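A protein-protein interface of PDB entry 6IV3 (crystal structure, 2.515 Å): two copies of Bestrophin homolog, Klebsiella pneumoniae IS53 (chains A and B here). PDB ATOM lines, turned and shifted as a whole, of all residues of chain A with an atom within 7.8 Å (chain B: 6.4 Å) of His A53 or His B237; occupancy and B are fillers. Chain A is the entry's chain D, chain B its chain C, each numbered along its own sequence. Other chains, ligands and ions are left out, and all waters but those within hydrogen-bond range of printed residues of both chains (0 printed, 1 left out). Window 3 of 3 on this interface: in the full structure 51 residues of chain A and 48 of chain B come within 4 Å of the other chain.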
ATOM      1  N   TYR A  47      18.362  -6.352  -4.257  1.00  0.00           N
ATOM      2  CA  TYR A  47      18.867  -5.309  -5.147  1.00  0.00           C
ATOM      3  C   TYR A  47      18.089  -5.216  -6.452  1.00  0.00           C
ATOM      4  O   TYR A  47      17.385  -4.231  -6.701  1.00  0.00           O
ATOM      5  CB  TYR A  47      20.336  -5.568  -5.480  1.00  0.00           C
ATOM      6  CG  TYR A  47      21.349  -4.666  -4.798  1.00  0.00           C
ATOM      7  CD1 TYR A  47      21.312  -4.440  -3.423  1.00  0.00           C
ATOM      8  CD2 TYR A  47      22.368  -4.069  -5.533  1.00  0.00           C
ATOM      9  CE1 TYR A  47      22.250  -3.633  -2.806  1.00  0.00           C
ATOM     10  CE2 TYR A  47      23.307  -3.267  -4.929  1.00  0.00           C
ATOM     11  CZ  TYR A  47      23.247  -3.048  -3.569  1.00  0.00           C
ATOM     12  OH  TYR A  47      24.199  -2.244  -2.987  1.00  0.00           O
ATOM     13  N   GLU A  48      18.252  -6.226  -7.310  1.00  0.00           N
ATOM     14  CA  GLU A  48      17.547  -6.241  -8.587  1.00  0.00           C
ATOM     15  C   GLU A  48      16.041  -6.358  -8.393  1.00  0.00           C
ATOM     16  O   GLU A  48      15.270  -5.866  -9.227  1.00  0.00           O
ATOM     17  CB  GLU A  48      18.072  -7.387  -9.457  1.00  0.00           C
ATOM     18  CG  GLU A  48      17.498  -7.425 -10.865  1.00  0.00           C
ATOM     19  CD  GLU A  48      18.547  -7.746 -11.919  1.00  0.00           C
ATOM     20  OE1 GLU A  48      19.253  -6.816 -12.385  1.00  0.00           O
ATOM     21  OE2 GLU A  48      18.660  -8.940 -12.284  1.00  0.00           O
ATOM     22  N   GLN A  49      15.602  -7.005  -7.306  1.00  0.00           N
ATOM     23  CA  GLN A  49      14.179  -7.019  -6.984  1.00  0.00           C
ATOM     24  C   GLN A  49      13.641  -5.598  -6.839  1.00  0.00           C
ATOM     25  O   GLN A  49      12.501  -5.316  -7.228  1.00  0.00           O
ATOM     26  CB  GLN A  49      13.932  -7.831  -5.710  1.00  0.00           C
ATOM     27  N   LEU A  50      14.457  -4.684  -6.302  1.00  0.00           N
ATOM     28  CA  LEU A  50      14.086  -3.275  -6.228  1.00  0.00           C
ATOM     29  C   LEU A  50      14.411  -2.488  -7.497  1.00  0.00           C
ATOM     30  O   LEU A  50      13.927  -1.360  -7.645  1.00  0.00           O
ATOM     31  CB  LEU A  50      14.771  -2.611  -5.028  1.00  0.00           C
ATOM     32  N   GLY A  51      15.202  -3.042  -8.414  1.00  0.00           N
ATOM     33  CA  GLY A  51      15.559  -2.341  -9.634  1.00  0.00           C
ATOM     34  C   GLY A  51      16.801  -1.479  -9.551  1.00  0.00           C
ATOM     35  O   GLY A  51      17.118  -0.779 -10.528  1.00  0.00           O
ATOM     36  N   ILE A  52      17.519  -1.515  -8.428  1.00  0.00           N
ATOM     37  CA  ILE A  52      18.712  -0.701  -8.227  1.00  0.00           C
ATOM     38  C   ILE A  52      19.938  -1.469  -8.724  1.00  0.00           C
ATOM     39  O   ILE A  52      20.235  -2.570  -8.245  1.00  0.00           O
ATOM     40  CB  ILE A  52      18.866  -0.285  -6.751  1.00  0.00           C
ATOM     41  CG1 ILE A  52      18.989  -1.489  -5.812  1.00  0.00           C
ATOM     42  CG2 ILE A  52      17.694   0.595  -6.315  1.00  0.00           C
ATOM     43  CD1 ILE A  52      20.097  -1.340  -4.791  1.00  0.00           C
ATOM     44  N   HIS A  53      20.632  -0.898  -9.706  1.00  0.00           N
ATOM     45  CA  HIS A  53      21.910  -1.414 -10.181  1.00  0.00           C
ATOM     46  C   HIS A  53      22.990  -0.377  -9.863  1.00  0.00           C
ATOM     47  O   HIS A  53      22.786   0.820 -10.098  1.00  0.00           O
ATOM     48  CB  HIS A  53      21.869  -1.725 -11.690  1.00  0.00           C
ATOM     49  CG  HIS A  53      20.720  -2.604 -12.123  1.00  0.00           C
ATOM     50  ND1 HIS A  53      19.830  -2.236 -13.113  1.00  0.00           N
ATOM     51  CD2 HIS A  53      20.336  -3.841 -11.724  1.00  0.00           C
ATOM     52  CE1 HIS A  53      18.940  -3.198 -13.294  1.00  0.00           C
ATOM     53  NE2 HIS A  53      19.226  -4.184 -12.465  1.00  0.00           N
ATOM     54  N   LEU A  54      24.125  -0.825  -9.308  1.00  0.00           N
ATOM     55  CA  LEU A  54      25.237   0.073  -8.979  1.00  0.00           C
ATOM     56  C   LEU A  54      26.570  -0.539  -9.390  1.00  0.00           C
ATOM     57  O   LEU A  54      27.007  -1.542  -8.818  1.00  0.00           O
ATOM     58  CB  LEU A  54      25.259   0.438  -7.492  1.00  0.00           C
ATOM     59  CG  LEU A  54      24.153   1.372  -6.986  1.00  0.00           C
ATOM     60  CD1 LEU A  54      24.318   1.627  -5.480  1.00  0.00           C
ATOM     61  CD2 LEU A  54      24.113   2.690  -7.775  1.00  0.00           C
ATOM     62  N   THR A  55      27.244   0.110 -10.335  1.00  0.00           N
ATOM     63  CA  THR A  55      28.546  -0.335 -10.792  1.00  0.00           C
ATOM     64  C   THR A  55      29.678   0.366 -10.033  1.00  0.00           C
ATOM     65  O   THR A  55      29.472   1.192  -9.135  1.00  0.00           O
ATOM     66  CB  THR A  55      28.694  -0.099 -12.295  1.00  0.00           C
ATOM     67  OG1 THR A  55      28.210   1.210 -12.626  1.00  0.00           O
ATOM     68  CG2 THR A  55      27.913  -1.152 -13.092  1.00  0.00           C
ATOM     69  N   PRO A  58      31.213   4.607 -12.181  1.00  0.00           N
ATOM     70  CA  PRO A  58      30.839   5.957 -11.728  1.00  0.00           C
ATOM     71  C   PRO A  58      31.537   6.360 -10.443  1.00  0.00           C
ATOM     72  O   PRO A  58      31.949   7.518 -10.290  1.00  0.00           O
ATOM     73  CB  PRO A  58      29.320   5.855 -11.543  1.00  0.00           C
ATOM     74  CG  PRO A  58      28.914   4.734 -12.457  1.00  0.00           C
ATOM     75  CD  PRO A  58      30.032   3.754 -12.397  1.00  0.00           C
ATOM     76  N   PHE A  59      31.694   5.423  -9.512  1.00  0.00           N
ATOM     77  CA  PHE A  59      32.378   5.750  -8.271  1.00  0.00           C
ATOM     78  C   PHE A  59      33.881   5.914  -8.479  1.00  0.00           C
ATOM     79  O   PHE A  59      34.519   6.668  -7.747  1.00  0.00           O
ATOM     80  CB  PHE A  59      32.076   4.693  -7.219  1.00  0.00           C
ATOM     81  CG  PHE A  59      30.737   4.870  -6.583  1.00  0.00           C
ATOM     82  CD1 PHE A  59      29.580   4.504  -7.264  1.00  0.00           C
ATOM     83  CD2 PHE A  59      30.622   5.443  -5.319  1.00  0.00           C
ATOM     84  CE1 PHE A  59      28.339   4.681  -6.695  1.00  0.00           C
ATOM     85  CE2 PHE A  59      29.382   5.624  -4.743  1.00  0.00           C
ATOM     86  CZ  PHE A  59      28.237   5.245  -5.432  1.00  0.00           C
ATOM     87  N   PHE A 230      28.187  -0.301  -1.319  1.00  0.00           N
ATOM     88  CA  PHE A 230      27.051  -0.700  -2.139  1.00  0.00           C
ATOM     89  C   PHE A 230      27.420  -0.766  -3.608  1.00  0.00           C
ATOM     90  O   PHE A 230      26.847  -1.567  -4.356  1.00  0.00           O
ATOM     91  CB  PHE A 230      25.884   0.257  -1.920  1.00  0.00           C
ATOM     92  CG  PHE A 230      25.359   0.230  -0.524  1.00  0.00           C
ATOM     93  CD1 PHE A 230      24.371  -0.673  -0.159  1.00  0.00           C
ATOM     94  CD2 PHE A 230      25.882   1.075   0.438  1.00  0.00           C
ATOM     95  CE1 PHE A 230      23.897  -0.714   1.138  1.00  0.00           C
ATOM     96  CE2 PHE A 230      25.417   1.039   1.736  1.00  0.00           C
ATOM     97  CZ  PHE A 230      24.424   0.143   2.093  1.00  0.00           C
ATOM     98  N   ALA A 231      28.372   0.059  -4.039  1.00  0.00           N
ATOM     99  CA  ALA A 231      28.852  -0.005  -5.410  1.00  0.00           C
ATOM    100  C   ALA A 231      29.906  -1.084  -5.605  1.00  0.00           C
ATOM    101  O   ALA A 231      30.126  -1.515  -6.740  1.00  0.00           O
ATOM    102  CB  ALA A 231      29.415   1.352  -5.830  1.00  0.00           C
ATOM    103  N   SER B  37      17.846  12.784 -15.420  1.00  0.00           N
ATOM    104  CA  SER B  37      17.979  11.353 -15.191  1.00  0.00           C
ATOM    105  C   SER B  37      16.638  10.651 -15.304  1.00  0.00           C
ATOM    106  O   SER B  37      16.584   9.484 -15.700  1.00  0.00           O
ATOM    107  CB  SER B  37      18.623  11.085 -13.832  1.00  0.00           C
ATOM    108  OG  SER B  37      17.905  11.738 -12.810  1.00  0.00           O
ATOM    109  N   ILE B  41      16.049   7.544 -17.690  1.00  0.00           N
ATOM    110  CA  ILE B  41      15.359   6.328 -17.263  1.00  0.00           C
ATOM    111  C   ILE B  41      14.197   6.011 -18.201  1.00  0.00           C
ATOM    112  O   ILE B  41      14.010   4.866 -18.624  1.00  0.00           O
ATOM    113  CB  ILE B  41      14.872   6.477 -15.809  1.00  0.00           C
ATOM    114  CG1 ILE B  41      16.021   6.289 -14.821  1.00  0.00           C
ATOM    115  CG2 ILE B  41      13.755   5.488 -15.519  1.00  0.00           C
ATOM    116  CD1 ILE B  41      15.627   6.549 -13.385  1.00  0.00           C
ATOM    117  N   TYR B  44      15.197   5.151 -22.001  1.00  0.00           N
ATOM    118  CA  TYR B  44      16.220   4.115 -22.256  1.00  0.00           C
ATOM    119  C   TYR B  44      15.660   3.017 -23.166  1.00  0.00           C
ATOM    120  O   TYR B  44      16.387   2.558 -24.033  1.00  0.00           O
ATOM    121  CB  TYR B  44      16.777   3.629 -20.920  1.00  0.00           C
ATOM    122  CG  TYR B  44      17.618   2.383 -20.936  1.00  0.00           C
ATOM    123  CD1 TYR B  44      17.425   1.403 -19.995  1.00  0.00           C
ATOM    124  CD2 TYR B  44      18.625   2.202 -21.851  1.00  0.00           C
ATOM    125  CE1 TYR B  44      18.196   0.263 -19.969  1.00  0.00           C
ATOM    126  CE2 TYR B  44      19.414   1.073 -21.839  1.00  0.00           C
ATOM    127  CZ  TYR B  44      19.201   0.095 -20.895  1.00  0.00           C
ATOM    128  OH  TYR B  44      19.977  -1.025 -20.855  1.00  0.00           O
ATOM    129  N   LEU B 232      24.716   7.050 -17.620  1.00  0.00           N
ATOM    130  CA  LEU B 232      24.625   6.184 -16.457  1.00  0.00           C
ATOM    131  C   LEU B 232      23.499   5.174 -16.552  1.00  0.00           C
ATOM    132  O   LEU B 232      23.559   4.140 -15.866  1.00  0.00           O
ATOM    133  CB  LEU B 232      24.431   7.020 -15.189  1.00  0.00           C
ATOM    134  CG  LEU B 232      25.650   7.853 -14.840  1.00  0.00           C
ATOM    135  CD1 LEU B 232      25.368   8.675 -13.580  1.00  0.00           C
ATOM    136  CD2 LEU B 232      26.845   6.922 -14.660  1.00  0.00           C
ATOM    137  N   VAL B 233      22.485   5.449 -17.381  1.00  0.00           N
ATOM    138  CA  VAL B 233      21.213   4.744 -17.251  1.00  0.00           C
ATOM    139  C   VAL B 233      21.342   3.285 -17.679  1.00  0.00           C
ATOM    140  O   VAL B 233      20.782   2.392 -17.038  1.00  0.00           O
ATOM    141  CB  VAL B 233      20.096   5.481 -18.015  1.00  0.00           C
ATOM    142  CG1 VAL B 233      20.369   5.538 -19.515  1.00  0.00           C
ATOM    143  CG2 VAL B 233      18.764   4.824 -17.725  1.00  0.00           C
ATOM    144  N   GLY B 234      22.095   3.013 -18.742  1.00  0.00           N
ATOM    145  CA  GLY B 234      22.299   1.636 -19.152  1.00  0.00           C
ATOM    146  C   GLY B 234      22.834   0.749 -18.045  1.00  0.00           C
ATOM    147  O   GLY B 234      22.509  -0.441 -17.987  1.00  0.00           O
ATOM    148  N   ASP B 235      23.638   1.313 -17.141  1.00  0.00           N
ATOM    149  CA  ASP B 235      24.287   0.565 -16.066  1.00  0.00           C
ATOM    150  C   ASP B 235      23.471   0.560 -14.783  1.00  0.00           C
ATOM    151  O   ASP B 235      23.420  -0.459 -14.091  1.00  0.00           O
ATOM    152  CB  ASP B 235      25.671   1.153 -15.756  1.00  0.00           C
ATOM    153  CG  ASP B 235      26.739   0.697 -16.727  1.00  0.00           C
ATOM    154  OD1 ASP B 235      26.637  -0.443 -17.245  1.00  0.00           O
ATOM    155  OD2 ASP B 235      27.658   1.502 -17.007  1.00  0.00           O
ATOM    156  N   LEU B 236      22.852   1.692 -14.438  1.00  0.00           N
ATOM    157  CA  LEU B 236      22.224   1.849 -13.131  1.00  0.00           C
ATOM    158  C   LEU B 236      20.716   1.666 -13.153  1.00  0.00           C
ATOM    159  O   LEU B 236      20.131   1.394 -12.097  1.00  0.00           O
ATOM    160  CB  LEU B 236      22.543   3.233 -12.546  1.00  0.00           C
ATOM    161  CG  LEU B 236      24.017   3.628 -12.441  1.00  0.00           C
ATOM    162  CD1 LEU B 236      24.156   4.928 -11.677  1.00  0.00           C
ATOM    163  CD2 LEU B 236      24.821   2.531 -11.773  1.00  0.00           C
ATOM    164  N   HIS B 237      20.087   1.803 -14.327  1.00  0.00           N
ATOM    165  CA  HIS B 237      18.638   1.758 -14.492  1.00  0.00           C
ATOM    166  C   HIS B 237      17.963   2.763 -13.566  1.00  0.00           C
ATOM    167  O   HIS B 237      18.015   3.972 -13.811  1.00  0.00           O
ATOM    168  CB  HIS B 237      18.105   0.345 -14.246  1.00  0.00           C
ATOM    169  CG  HIS B 237      18.374  -0.614 -15.367  1.00  0.00           C
ATOM    170  ND1 HIS B 237      19.325  -0.383 -16.338  1.00  0.00           N
ATOM    171  CD2 HIS B 237      17.805  -1.806 -15.676  1.00  0.00           C
ATOM    172  CE1 HIS B 237      19.340  -1.395 -17.187  1.00  0.00           C
ATOM    173  NE2 HIS B 237      18.428  -2.272 -16.809  1.00  0.00           N
ATOM    174  N   TYR B 238      17.340   2.283 -12.489  1.00  0.00           N
ATOM    175  CA  TYR B 238      16.603   3.172 -11.597  1.00  0.00           C
ATOM    176  C   TYR B 238      17.483   3.873 -10.578  1.00  0.00           C
ATOM    177  O   TYR B 238      16.970   4.710  -9.830  1.00  0.00           O
ATOM    178  CB  TYR B 238      15.495   2.406 -10.864  1.00  0.00           C
ATOM    179  CG  TYR B 238      14.286   2.160 -11.735  1.00  0.00           C
ATOM    180  CD1 TYR B 238      13.245   1.352 -11.313  1.00  0.00           C
ATOM    181  CD2 TYR B 238      14.201   2.738 -12.997  1.00  0.00           C
ATOM    182  CE1 TYR B 238      12.144   1.139 -12.123  1.00  0.00           C
ATOM    183  CE2 TYR B 238      13.114   2.529 -13.808  1.00  0.00           C
ATOM    184  CZ  TYR B 238      12.087   1.730 -13.371  1.00  0.00           C
ATOM    185  OH  TYR B 238      11.001   1.521 -14.192  1.00  0.00           O
ATOM    186  N   MET B 239      18.776   3.546 -10.522  1.00  0.00           N
ATOM    187  CA  MET B 239      19.717   4.236  -9.645  1.00  0.00           C
ATOM    188  C   MET B 239      20.326   5.474 -10.288  1.00  0.00           C
ATOM    189  O   MET B 239      20.909   6.308  -9.579  1.00  0.00           O
ATOM    190  CB  MET B 239      20.842   3.285  -9.222  1.00  0.00           C
ATOM    191  CG  MET B 239      20.525   2.452  -7.999  1.00  0.00           C
ATOM    192  SD  MET B 239      19.968   3.435  -6.599  1.00  0.00           S
ATOM    193  CE  MET B 239      21.408   4.474  -6.379  1.00  0.00           C
ATOM    194  N   THR B 240      20.192   5.613 -11.608  1.00  0.00           N
ATOM    195  CA  THR B 240      20.709   6.772 -12.340  1.00  0.00           C
ATOM    196  C   THR B 240      20.514   8.114 -11.638  1.00  0.00           C
ATOM    197  O   THR B 240      21.478   8.888 -11.586  1.00  0.00           O
ATOM    198  CB  THR B 240      20.075   6.765 -13.738  1.00  0.00           C
ATOM    199  OG1 THR B 240      20.464   5.560 -14.401  1.00  0.00           O
ATOM    200  CG2 THR B 240      20.548   7.954 -14.554  1.00  0.00           C
ATOM    201  N   PRO B 241      19.347   8.444 -11.061  1.00  0.00           N
ATOM    202  CA  PRO B 241      19.200   9.794 -10.485  1.00  0.00           C
ATOM    203  C   PRO B 241      20.068  10.040  -9.266  1.00  0.00           C
ATOM    204  O   PRO B 241      20.606  11.144  -9.115  1.00  0.00           O
ATOM    205  CB  PRO B 241      17.704   9.863 -10.141  1.00  0.00           C
ATOM    206  CG  PRO B 241      17.323   8.440  -9.909  1.00  0.00           C
ATOM    207  CD  PRO B 241      18.082   7.688 -10.954  1.00  0.00           C
ATOM    208  N   VAL B 243      23.064   8.521  -8.172  1.00  0.00           N
ATOM    209  CA  VAL B 243      24.475   8.639  -8.521  1.00  0.00           C
ATOM    210  C   VAL B 243      24.710   9.885  -9.370  1.00  0.00           C
ATOM    211  O   VAL B 243      25.648  10.658  -9.121  1.00  0.00           O
ATOM    212  CB  VAL B 243      24.939   7.346  -9.216  1.00  0.00           C
ATOM    213  CG1 VAL B 243      26.325   7.492  -9.796  1.00  0.00           C
ATOM    214  CG2 VAL B 243      24.900   6.195  -8.216  1.00  0.00           C
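Of the printed residues of chain A, His B237 touches His A53 (3.0 Å). Printed residues of chain B within 4 Å of Pro A58: Leu B232 (3.7 Å) and Val B243 (3.8 Å). Of the printed residues of chain A, Leu B236 touches His A53 (3.1 Å), Leu A54 (3.7 Å) and Thr A55 (3.7 Å). Thr B240 touches none of the printed residues of chain A. The nearest printed residue of chain A that does not touch His B237 is Gly A51 (4.01 Å).
Hydrophobic or aromatic side chains of chain B within 4 Å of the printed part of chain A: Leu B232, Leu B236, His B237, Tyr B238, Met B239 and Val B243. Along chain B the printed residues that touch a printed residue of chain A span positions 232 to 243. Among the printed residues, 12 pairs touch across the chains. Among the printed residues, no Asp or Glu carboxylate lies within 4 Å of a Lys or Arg side-chain nitrogen of the other chain.
No position is printed for both chains. Of the 12 pairs that touch across the chains among the printed residues, none has its exchanged pair printed and touching as well.
The backbone carbonyl oxygen (O) of Val B233 lies within hydrogen-bond range of a ring nitrogen (ND1) of His B237, at 3.2 Å. The backbone NH (N) of Ile A52 is in hydrogen-bond range of the backbone carbonyl oxygen (O) of Tyr A47, 3.2 Å away. The side-chain hydroxyl (OG1) of Thr B240 is in hydrogen-bond range of the backbone carbonyl oxygen (O) of His B237. OE1 of Glu A48 lies within hydrogen-bond range of NE2 of His A53 (2.6 Å).
Gly A51 touches Tyr B238 (O to CB, 3.6 Å). Met B239 touches Ile A52 (CG to CB, 3.4 Å). Asp B235 touches His A53 (O to CB, 3.1 Å). CE1 of His A53 touches CD2 of His B237 (3.0 Å). His A53 touches Met B239 (O to CB, 3.3 Å). Leu A54 touches Leu B236. Met B239 touches Leu A54 (CE to CD2, 3.5 Å). Val B243 touches Leu A54. Leu B232 touches Pro A58. CG1 of Val B243 touches CB of Pro A58, 3.8 Å away.
O of Leu B236 lies within hydrogen-bond range of N of His A53 (3.3 Å).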
